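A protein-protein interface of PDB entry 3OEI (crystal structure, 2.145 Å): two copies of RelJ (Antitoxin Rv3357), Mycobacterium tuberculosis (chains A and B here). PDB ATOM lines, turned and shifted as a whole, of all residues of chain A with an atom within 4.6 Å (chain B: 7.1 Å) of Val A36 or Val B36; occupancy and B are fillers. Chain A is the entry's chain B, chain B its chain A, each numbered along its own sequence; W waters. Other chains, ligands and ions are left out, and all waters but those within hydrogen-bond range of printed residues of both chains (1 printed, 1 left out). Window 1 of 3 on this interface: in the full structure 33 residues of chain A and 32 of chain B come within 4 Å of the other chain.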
ATOM      1  N   PRO A  25      -3.368  17.767  17.664  1.00  0.00           N
ATOM      2  CA  PRO A  25      -2.064  18.437  17.666  1.00  0.00           C
ATOM      3  C   PRO A  25      -2.203  19.933  17.947  1.00  0.00           C
ATOM      4  O   PRO A  25      -3.215  20.535  17.590  1.00  0.00           O
ATOM      5  CB  PRO A  25      -1.563  18.206  16.235  1.00  0.00           C
ATOM      6  CG  PRO A  25      -2.291  16.945  15.780  1.00  0.00           C
ATOM      7  CD  PRO A  25      -3.645  17.075  16.391  1.00  0.00           C
ATOM      8  N   VAL A  26      -1.227  20.546  18.593  1.00  0.00           N
ATOM      9  CA  VAL A  26      -1.301  22.006  18.673  1.00  0.00           C
ATOM     10  C   VAL A  26      -0.148  22.692  17.961  1.00  0.00           C
ATOM     11  O   VAL A  26       1.008  22.280  18.054  1.00  0.00           O
ATOM     12  CB  VAL A  26      -1.559  22.574  20.118  1.00  0.00           C
ATOM     13  CG1 VAL A  26      -1.785  21.461  21.130  1.00  0.00           C
ATOM     14  CG2 VAL A  26      -0.457  23.538  20.551  1.00  0.00           C
ATOM     15  N   ARG A  27      -0.497  23.735  17.232  1.00  0.00           N
ATOM     16  CA  ARG A  27       0.458  24.499  16.451  1.00  0.00           C
ATOM     17  C   ARG A  27       1.074  25.605  17.295  1.00  0.00           C
ATOM     18  O   ARG A  27       0.396  26.266  18.083  1.00  0.00           O
ATOM     19  CB  ARG A  27      -0.222  25.068  15.187  1.00  0.00           C
ATOM     20  CG  ARG A  27       0.753  25.611  14.115  1.00  0.00           C
ATOM     21  CD  ARG A  27       0.038  25.899  12.764  1.00  0.00           C
ATOM     22  NE  ARG A  27      -0.579  24.688  12.233  1.00  0.00           N
ATOM     23  CZ  ARG A  27      -0.084  23.965  11.230  1.00  0.00           C
ATOM     24  NH1 ARG A  27       1.029  24.343  10.605  1.00  0.00           N
ATOM     25  NH2 ARG A  27      -0.717  22.867  10.837  1.00  0.00           N
ATOM     26  N   ALA A  35       6.103  25.295  14.737  1.00  0.00           N
ATOM     27  CA  ALA A  35       6.218  23.897  15.085  1.00  0.00           C
ATOM     28  C   ALA A  35       4.836  23.367  15.436  1.00  0.00           C
ATOM     29  O   ALA A  35       3.877  24.147  15.628  1.00  0.00           O
ATOM     30  CB  ALA A  35       7.156  23.736  16.251  1.00  0.00           C
ATOM     31  N   VAL A  36       4.751  22.043  15.512  1.00  0.00           N
ATOM     32  CA  VAL A  36       3.529  21.344  15.875  1.00  0.00           C
ATOM     33  C   VAL A  36       3.879  20.272  16.882  1.00  0.00           C
ATOM     34  O   VAL A  36       4.849  19.526  16.696  1.00  0.00           O
ATOM     35  CB  VAL A  36       2.848  20.706  14.623  1.00  0.00           C
ATOM     36  CG1 VAL A  36       1.718  19.759  15.021  1.00  0.00           C
ATOM     37  CG2 VAL A  36       2.331  21.793  13.687  1.00  0.00           C
ATOM     38  N   LEU A  37       3.107  20.217  17.968  1.00  0.00           N
ATOM     39  CA  LEU A  37       3.311  19.209  18.983  1.00  0.00           C
ATOM     40  C   LEU A  37       2.154  18.227  18.918  1.00  0.00           C
ATOM     41  O   LEU A  37       1.002  18.630  18.844  1.00  0.00           O
ATOM     42  CB  LEU A  37       3.357  19.864  20.369  1.00  0.00           C
ATOM     43  CG  LEU A  37       3.548  18.908  21.552  1.00  0.00           C
ATOM     44  CD1 LEU A  37       5.036  18.512  21.710  1.00  0.00           C
ATOM     45  CD2 LEU A  37       3.012  19.522  22.841  1.00  0.00           C
ATOM     46  N   MET A  38       2.445  16.938  18.973  1.00  0.00           N
ATOM     47  CA  MET A  38       1.380  15.949  18.830  1.00  0.00           C
ATOM     48  C   MET A  38       1.695  14.716  19.629  1.00  0.00           C
ATOM     49  O   MET A  38       2.834  14.497  20.031  1.00  0.00           O
ATOM     50  CB  MET A  38       1.170  15.585  17.343  1.00  0.00           C
ATOM     51  CG  MET A  38       2.299  14.731  16.769  1.00  0.00           C
ATOM     52  SD  MET A  38       2.117  14.261  15.003  1.00  0.00           S
ATOM     53  CE  MET A  38       0.486  13.491  14.996  1.00  0.00           C
ATOM     54  N   SER A  39       0.669  13.910  19.852  1.00  0.00           N
ATOM     55  CA  SER A  39       0.794  12.583  20.449  1.00  0.00           C
ATOM     56  C   SER A  39       1.797  11.690  19.723  1.00  0.00           C
ATOM     57  O   SER A  39       1.653  11.447  18.534  1.00  0.00           O
ATOM     58  CB  SER A  39      -0.584  11.889  20.427  1.00  0.00           C
ATOM     59  OG  SER A  39      -0.493  10.514  20.756  1.00  0.00           O
ATOM     60  N   ALA A  40       2.792  11.187  20.454  1.00  0.00           N
ATOM     61  CA  ALA A  40       3.740  10.239  19.903  1.00  0.00           C
ATOM     62  C   ALA A  40       3.021   8.952  19.464  1.00  0.00           C
ATOM     63  O   ALA A  40       3.317   8.404  18.392  1.00  0.00           O
ATOM     64  CB  ALA A  40       4.831   9.917  20.922  1.00  0.00           C
ATOM     65  N   TYR A  43       1.178   9.598  16.209  1.00  0.00           N
ATOM     66  CA  TYR A  43       2.202   9.676  15.183  1.00  0.00           C
ATOM     67  C   TYR A  43       2.678   8.295  14.741  1.00  0.00           C
ATOM     68  O   TYR A  43       2.637   7.981  13.552  1.00  0.00           O
ATOM     69  CB  TYR A  43       3.372  10.527  15.649  1.00  0.00           C
ATOM     70  CG  TYR A  43       4.477  10.540  14.639  1.00  0.00           C
ATOM     71  CD1 TYR A  43       4.367  11.298  13.478  1.00  0.00           C
ATOM     72  CD2 TYR A  43       5.598   9.750  14.808  1.00  0.00           C
ATOM     73  CE1 TYR A  43       5.360  11.304  12.538  1.00  0.00           C
ATOM     74  CE2 TYR A  43       6.612   9.750  13.870  1.00  0.00           C
ATOM     75  CZ  TYR A  43       6.485  10.532  12.739  1.00  0.00           C
ATOM     76  OH  TYR A  43       7.487  10.543  11.805  1.00  0.00           O
ATOM     77  N   ILE B  16      12.588  24.250  18.840  1.00  0.00           N
ATOM     78  CA  ILE B  16      11.832  24.742  17.696  1.00  0.00           C
ATOM     79  C   ILE B  16      12.743  25.216  16.539  1.00  0.00           C
ATOM     80  O   ILE B  16      12.478  24.900  15.377  1.00  0.00           O
ATOM     81  CB  ILE B  16      10.821  25.836  18.119  1.00  0.00           C
ATOM     82  CG1 ILE B  16       9.723  25.227  18.995  1.00  0.00           C
ATOM     83  CG2 ILE B  16      10.190  26.528  16.892  1.00  0.00           C
ATOM     84  CD1 ILE B  16       8.847  26.260  19.629  1.00  0.00           C
ATOM     85  N   VAL B  19      14.095  21.849  14.846  1.00  0.00           N
ATOM     86  CA  VAL B  19      13.226  21.050  13.988  1.00  0.00           C
ATOM     87  C   VAL B  19      12.985  21.773  12.661  1.00  0.00           C
ATOM     88  O   VAL B  19      12.782  21.139  11.628  1.00  0.00           O
ATOM     89  CB  VAL B  19      11.893  20.610  14.699  1.00  0.00           C
ATOM     90  CG1 VAL B  19      12.213  19.774  15.968  1.00  0.00           C
ATOM     91  CG2 VAL B  19      11.021  21.809  15.039  1.00  0.00           C
ATOM     92  N   GLN B  24      13.894  16.958  11.386  1.00  0.00           N
ATOM     93  CA  GLN B  24      13.716  15.687  12.061  1.00  0.00           C
ATOM     94  C   GLN B  24      12.827  15.912  13.277  1.00  0.00           C
ATOM     95  O   GLN B  24      13.038  16.852  14.044  1.00  0.00           O
ATOM     96  CB  GLN B  24      15.048  15.105  12.539  1.00  0.00           C
ATOM     97  CG  GLN B  24      16.090  14.957  11.461  1.00  0.00           C
ATOM     98  CD  GLN B  24      15.551  14.229  10.253  1.00  0.00           C
ATOM     99  OE1 GLN B  24      15.276  13.033  10.314  1.00  0.00           O
ATOM    100  NE2 GLN B  24      15.361  14.958   9.159  1.00  0.00           N
ATOM    101  N   PRO B  25      11.830  15.052  13.458  1.00  0.00           N
ATOM    102  CA  PRO B  25      10.977  15.149  14.646  1.00  0.00           C
ATOM    103  C   PRO B  25      11.773  14.918  15.937  1.00  0.00           C
ATOM    104  O   PRO B  25      12.687  14.083  15.949  1.00  0.00           O
ATOM    105  CB  PRO B  25       9.997  13.984  14.464  1.00  0.00           C
ATOM    106  CG  PRO B  25      10.015  13.700  12.991  1.00  0.00           C
ATOM    107  CD  PRO B  25      11.404  13.987  12.537  1.00  0.00           C
ATOM    108  N   VAL B  26      11.410  15.631  17.002  1.00  0.00           N
ATOM    109  CA  VAL B  26      11.937  15.380  18.348  1.00  0.00           C
ATOM    110  C   VAL B  26      10.928  14.631  19.236  1.00  0.00           C
ATOM    111  O   VAL B  26       9.788  15.077  19.408  1.00  0.00           O
ATOM    112  CB  VAL B  26      12.327  16.708  19.024  1.00  0.00           C
ATOM    113  CG1 VAL B  26      12.597  16.515  20.521  1.00  0.00           C
ATOM    114  CG2 VAL B  26      13.527  17.287  18.320  1.00  0.00           C
ATOM    115  N   ARG B  27      11.338  13.502  19.809  1.00  0.00           N
ATOM    116  CA  ARG B  27      10.429  12.747  20.660  1.00  0.00           C
ATOM    117  C   ARG B  27      10.580  13.149  22.128  1.00  0.00           C
ATOM    118  O   ARG B  27      11.676  13.187  22.651  1.00  0.00           O
ATOM    119  CB  ARG B  27      10.618  11.234  20.478  1.00  0.00           C
ATOM    120  CG  ARG B  27       9.560  10.395  21.179  1.00  0.00           C
ATOM    121  CD  ARG B  27       9.613   8.916  20.754  1.00  0.00           C
ATOM    122  NE  ARG B  27       9.383   8.739  19.317  1.00  0.00           N
ATOM    123  CZ  ARG B  27       8.306   8.152  18.786  1.00  0.00           C
ATOM    124  NH1 ARG B  27       7.348   7.676  19.566  1.00  0.00           N
ATOM    125  NH2 ARG B  27       8.192   8.027  17.467  1.00  0.00           N
ATOM    126  N   ILE B  28       9.461  13.437  22.787  1.00  0.00           N
ATOM    127  CA  ILE B  28       9.466  13.929  24.170  1.00  0.00           C
ATOM    128  C   ILE B  28       8.722  12.943  25.075  1.00  0.00           C
ATOM    129  O   ILE B  28       7.584  12.563  24.788  1.00  0.00           O
ATOM    130  CB  ILE B  28       8.791  15.312  24.261  1.00  0.00           C
ATOM    131  CG1 ILE B  28       9.411  16.269  23.252  1.00  0.00           C
ATOM    132  CG2 ILE B  28       8.873  15.915  25.697  1.00  0.00           C
ATOM    133  CD1 ILE B  28       8.770  17.640  23.265  1.00  0.00           C
ATOM    134  N   ASP B  34       3.876  10.339  25.780  1.00  0.00           N
ATOM    135  CA  ASP B  34       4.933  10.885  24.954  1.00  0.00           C
ATOM    136  C   ASP B  34       4.360  11.755  23.847  1.00  0.00           C
ATOM    137  O   ASP B  34       3.199  11.604  23.424  1.00  0.00           O
ATOM    138  CB  ASP B  34       5.800   9.771  24.367  1.00  0.00           C
ATOM    139  CG  ASP B  34       6.627   9.051  25.422  1.00  0.00           C
ATOM    140  OD1 ASP B  34       7.179   7.986  25.089  1.00  0.00           O
ATOM    141  OD2 ASP B  34       6.732   9.540  26.574  1.00  0.00           O
ATOM    142  N   ALA B  35       5.189  12.676  23.388  1.00  0.00           N
ATOM    143  CA  ALA B  35       4.804  13.598  22.335  1.00  0.00           C
ATOM    144  C   ALA B  35       5.903  13.666  21.273  1.00  0.00           C
ATOM    145  O   ALA B  35       7.060  13.339  21.559  1.00  0.00           O
ATOM    146  CB  ALA B  35       4.553  14.961  22.912  1.00  0.00           C
ATOM    147  N   VAL B  36       5.523  14.075  20.060  1.00  0.00           N
ATOM    148  CA  VAL B  36       6.477  14.391  19.014  1.00  0.00           C
ATOM    149  C   VAL B  36       6.379  15.875  18.696  1.00  0.00           C
ATOM    150  O   VAL B  36       5.284  16.410  18.556  1.00  0.00           O
ATOM    151  CB  VAL B  36       6.228  13.526  17.738  1.00  0.00           C
ATOM    152  CG1 VAL B  36       7.017  14.058  16.556  1.00  0.00           C
ATOM    153  CG2 VAL B  36       6.581  12.078  18.004  1.00  0.00           C
ATOM    154  N   LEU B  37       7.528  16.548  18.629  1.00  0.00           N
ATOM    155  CA  LEU B  37       7.613  17.927  18.173  1.00  0.00           C
ATOM    156  C   LEU B  37       8.189  17.953  16.748  1.00  0.00           C
ATOM    157  O   LEU B  37       9.254  17.388  16.495  1.00  0.00           O
ATOM    158  CB  LEU B  37       8.548  18.726  19.074  1.00  0.00           C
ATOM    159  CG  LEU B  37       8.705  20.193  18.689  1.00  0.00           C
ATOM    160  CD1 LEU B  37       7.412  20.923  18.924  1.00  0.00           C
ATOM    161  CD2 LEU B  37       9.859  20.870  19.466  1.00  0.00           C
ATOM    162  N   MET B  38       7.502  18.607  15.818  1.00  0.00           N
ATOM    163  CA  MET B  38       8.064  18.792  14.474  1.00  0.00           C
ATOM    164  C   MET B  38       7.848  20.200  13.962  1.00  0.00           C
ATOM    165  O   MET B  38       7.032  20.931  14.497  1.00  0.00           O
ATOM    166  CB  MET B  38       7.558  17.729  13.478  1.00  0.00           C
ATOM    167  CG  MET B  38       6.081  17.406  13.571  1.00  0.00           C
ATOM    168  SD  MET B  38       5.578  16.106  12.403  1.00  0.00           S
ATOM    169  CE  MET B  38       6.702  16.504  11.090  1.00  0.00           C
ATOM    170  N   SER B  39       8.610  20.600  12.954  1.00  0.00           N
ATOM    171  CA  SER B  39       8.343  21.888  12.332  1.00  0.00           C
ATOM    172  C   SER B  39       6.948  21.887  11.702  1.00  0.00           C
ATOM    173  O   SER B  39       6.421  20.828  11.325  1.00  0.00           O
ATOM    174  CB  SER B  39       9.408  22.246  11.284  1.00  0.00           C
ATOM    175  OG  SER B  39       9.209  21.530  10.081  1.00  0.00           O
ATOM    176  N   ALA B  40       6.346  23.073  11.607  1.00  0.00           N
ATOM    177  CA  ALA B  40       5.020  23.194  11.023  1.00  0.00           C
ATOM    178  C   ALA B  40       5.026  22.757   9.542  1.00  0.00           C
ATOM    179  O   ALA B  40       4.111  22.061   9.073  1.00  0.00           O
ATOM    180  CB  ALA B  40       4.497  24.618  11.179  1.00  0.00           C
ATOM    181  N   ASP B  41       6.071  23.152   8.820  1.00  0.00           N
ATOM    182  CA  ASP B  41       6.236  22.747   7.426  1.00  0.00           C
ATOM    183  C   ASP B  41       6.312  21.230   7.310  1.00  0.00           C
ATOM    184  O   ASP B  41       5.599  20.639   6.495  1.00  0.00           O
ATOM    185  CB  ASP B  41       7.478  23.384   6.805  1.00  0.00           C
ATOM    186  CG  ASP B  41       7.305  24.874   6.554  1.00  0.00           C
ATOM    187  OD1 ASP B  41       6.142  25.334   6.498  1.00  0.00           O
ATOM    188  OD2 ASP B  41       8.328  25.582   6.408  1.00  0.00           O
ATOM    189  N   TYR B  43       5.296  18.961   9.483  1.00  0.00           N
ATOM    190  CA  TYR B  43       4.032  18.389   9.875  1.00  0.00           C
ATOM    191  C   TYR B  43       3.019  18.439   8.728  1.00  0.00           C
ATOM    192  O   TYR B  43       2.312  17.458   8.504  1.00  0.00           O
ATOM    193  CB  TYR B  43       3.470  19.055  11.120  1.00  0.00           C
ATOM    194  CG  TYR B  43       2.064  18.590  11.453  1.00  0.00           C
ATOM    195  CD1 TYR B  43       1.841  17.391  12.102  1.00  0.00           C
ATOM    196  CD2 TYR B  43       0.968  19.379  11.144  1.00  0.00           C
ATOM    197  CE1 TYR B  43       0.558  16.969  12.400  1.00  0.00           C
ATOM    198  CE2 TYR B  43      -0.314  18.971  11.439  1.00  0.00           C
ATOM    199  CZ  TYR B  43      -0.520  17.770  12.062  1.00  0.00           C
ATOM    200  OH  TYR B  43      -1.813  17.386  12.358  1.00  0.00           O
ATOM    201  N   ASP B  44       2.950  19.567   8.016  1.00  0.00           N
ATOM    202  CA  ASP B  44       2.028  19.689   6.879  1.00  0.00           C
ATOM    203  C   ASP B  44       2.359  18.662   5.777  1.00  0.00           C
ATOM    204  O   ASP B  44       1.462  18.030   5.214  1.00  0.00           O
ATOM    205  CB  ASP B  44       2.028  21.101   6.282  1.00  0.00           C
ATOM    206  CG  ASP B  44       1.473  22.164   7.248  1.00  0.00           C
ATOM    207  OD1 ASP B  44       0.776  21.804   8.213  1.00  0.00           O
ATOM    208  OD2 ASP B  44       1.735  23.373   7.032  1.00  0.00           O
HETATM  209  O   HOH W   1       1.762   9.345  22.967  1.00  0.00           O
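N of Ala A40 lies within hydrogen-bond range of O of Asp B34 (3.0 Å). N of Val B36 is in hydrogen-bond range of O of Met A38 (2.7 Å). The backbone carbonyl oxygen (O) of Met B38 lies within hydrogen-bond range of the backbone NH (N) of Val A36 (2.7 Å). The side-chain carboxylate (OD1) of Asp B44 lies within salt-bridge range of the guanidinium group (NH2) of Arg A27, 3.2 Å away.
O of Val B26 sits at hydrogen-bond distance from N of Leu B37 (2.8 Å). The backbone carbonyl oxygen of Ala B35 sits at hydrogen-bond distance from the backbone NH of Ile B28 (2.7 Å). N of Leu A37 sits at hydrogen-bond distance from O of Val A26 (2.9 Å).
Arg A27 touches Ala B40. NH2 of Arg A27 touches CD2 of Tyr B43 (3.9 Å). Ala A35 touches Leu B37. Ala A35 touches Met B38 (CA to O, 3.1 Å). N of Ala B40 touches CA of Ala A35, at 3.6 Å. Val A36 touches Leu B37 (O to CA, 3.5 Å). Ala B35 touches Leu A37. Val B36 touches Leu A37. Arg B27 touches Ala A40. Ala A40 touches Ala B35.
Of chain B, only Val B36, Leu B37, Met B38 and Tyr B43 come within 4 Å of Val A36. Printed residues of chain A within 4 Å of Val B36: Val A36 (3.7 Å), Leu A37 (3.5 Å), Met A38 (2.7 Å) and Ala A40 (3.9 Å). Of the printed residues of chain A, Leu B37 touches Ala A35 and Val A36. Of the printed residues of chain A, Arg B27 touches Ala A40. Printed residues of chain B within 4 Å of Leu A37: Ala B35 and Val B36. Of the printed residues of chain B, Pro A25 touches Tyr B43 (3.5 Å). Asp B41 touches none of the printed residues of chain A. The nearest residue of chain B that does not touch Val A36 is Ala B40 (4.04 Å). The nearest residue of chain A that does not touch Val B36 is Tyr A43 (4.1 Å).
Hydrophobic or aromatic side chains of chain A within 4 Å of the printed part of chain B: Pro A25, Ala A35, Val A36, Leu A37, Met A38 and Ala A40. Printed residues of chain B that touch a printed residue of chain A: Arg B27, Asp B34, Ala B35, Val B36, Leu B37, Met B38, Ala B40, Tyr B43 and Asp B44. Hydrophobic or aromatic side chains of chain B within 4 Å of the printed part of chain A: Ala B35, Val B36, Leu B37, Met B38, Ala B40 and Tyr B43.
Pro A25 touches Tyr B43, but with the chains exchanged Tyr A43 does not touch Pro B25 (4.2 Å). Ala A35 touches Leu B37, and with the chains exchanged Leu A37 touches Ala B35. Ala A35 touches Met B38, and with the chains exchanged Met A38 touches Ala B35. Val A36 touches Met B38, and with the chains exchanged Met A38 touches Val B36. Positions printed for both chains: 25, 26, 27, 35, 36, 37, 38, 39, 40 and 43. Of the 20 pairs that touch across the chains among the printed residues, 13 have their exchanged pair printed and touching as well.
Water W1 lies within hydrogen-bond range of the backbone carbonyl oxygen (O) of Asp B34 (2.7 Å), the backbone NH (N) of Ala A40 (3.3 Å) and the side-chain hydroxyl (OG) of Ser A39 (3.4 Å).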
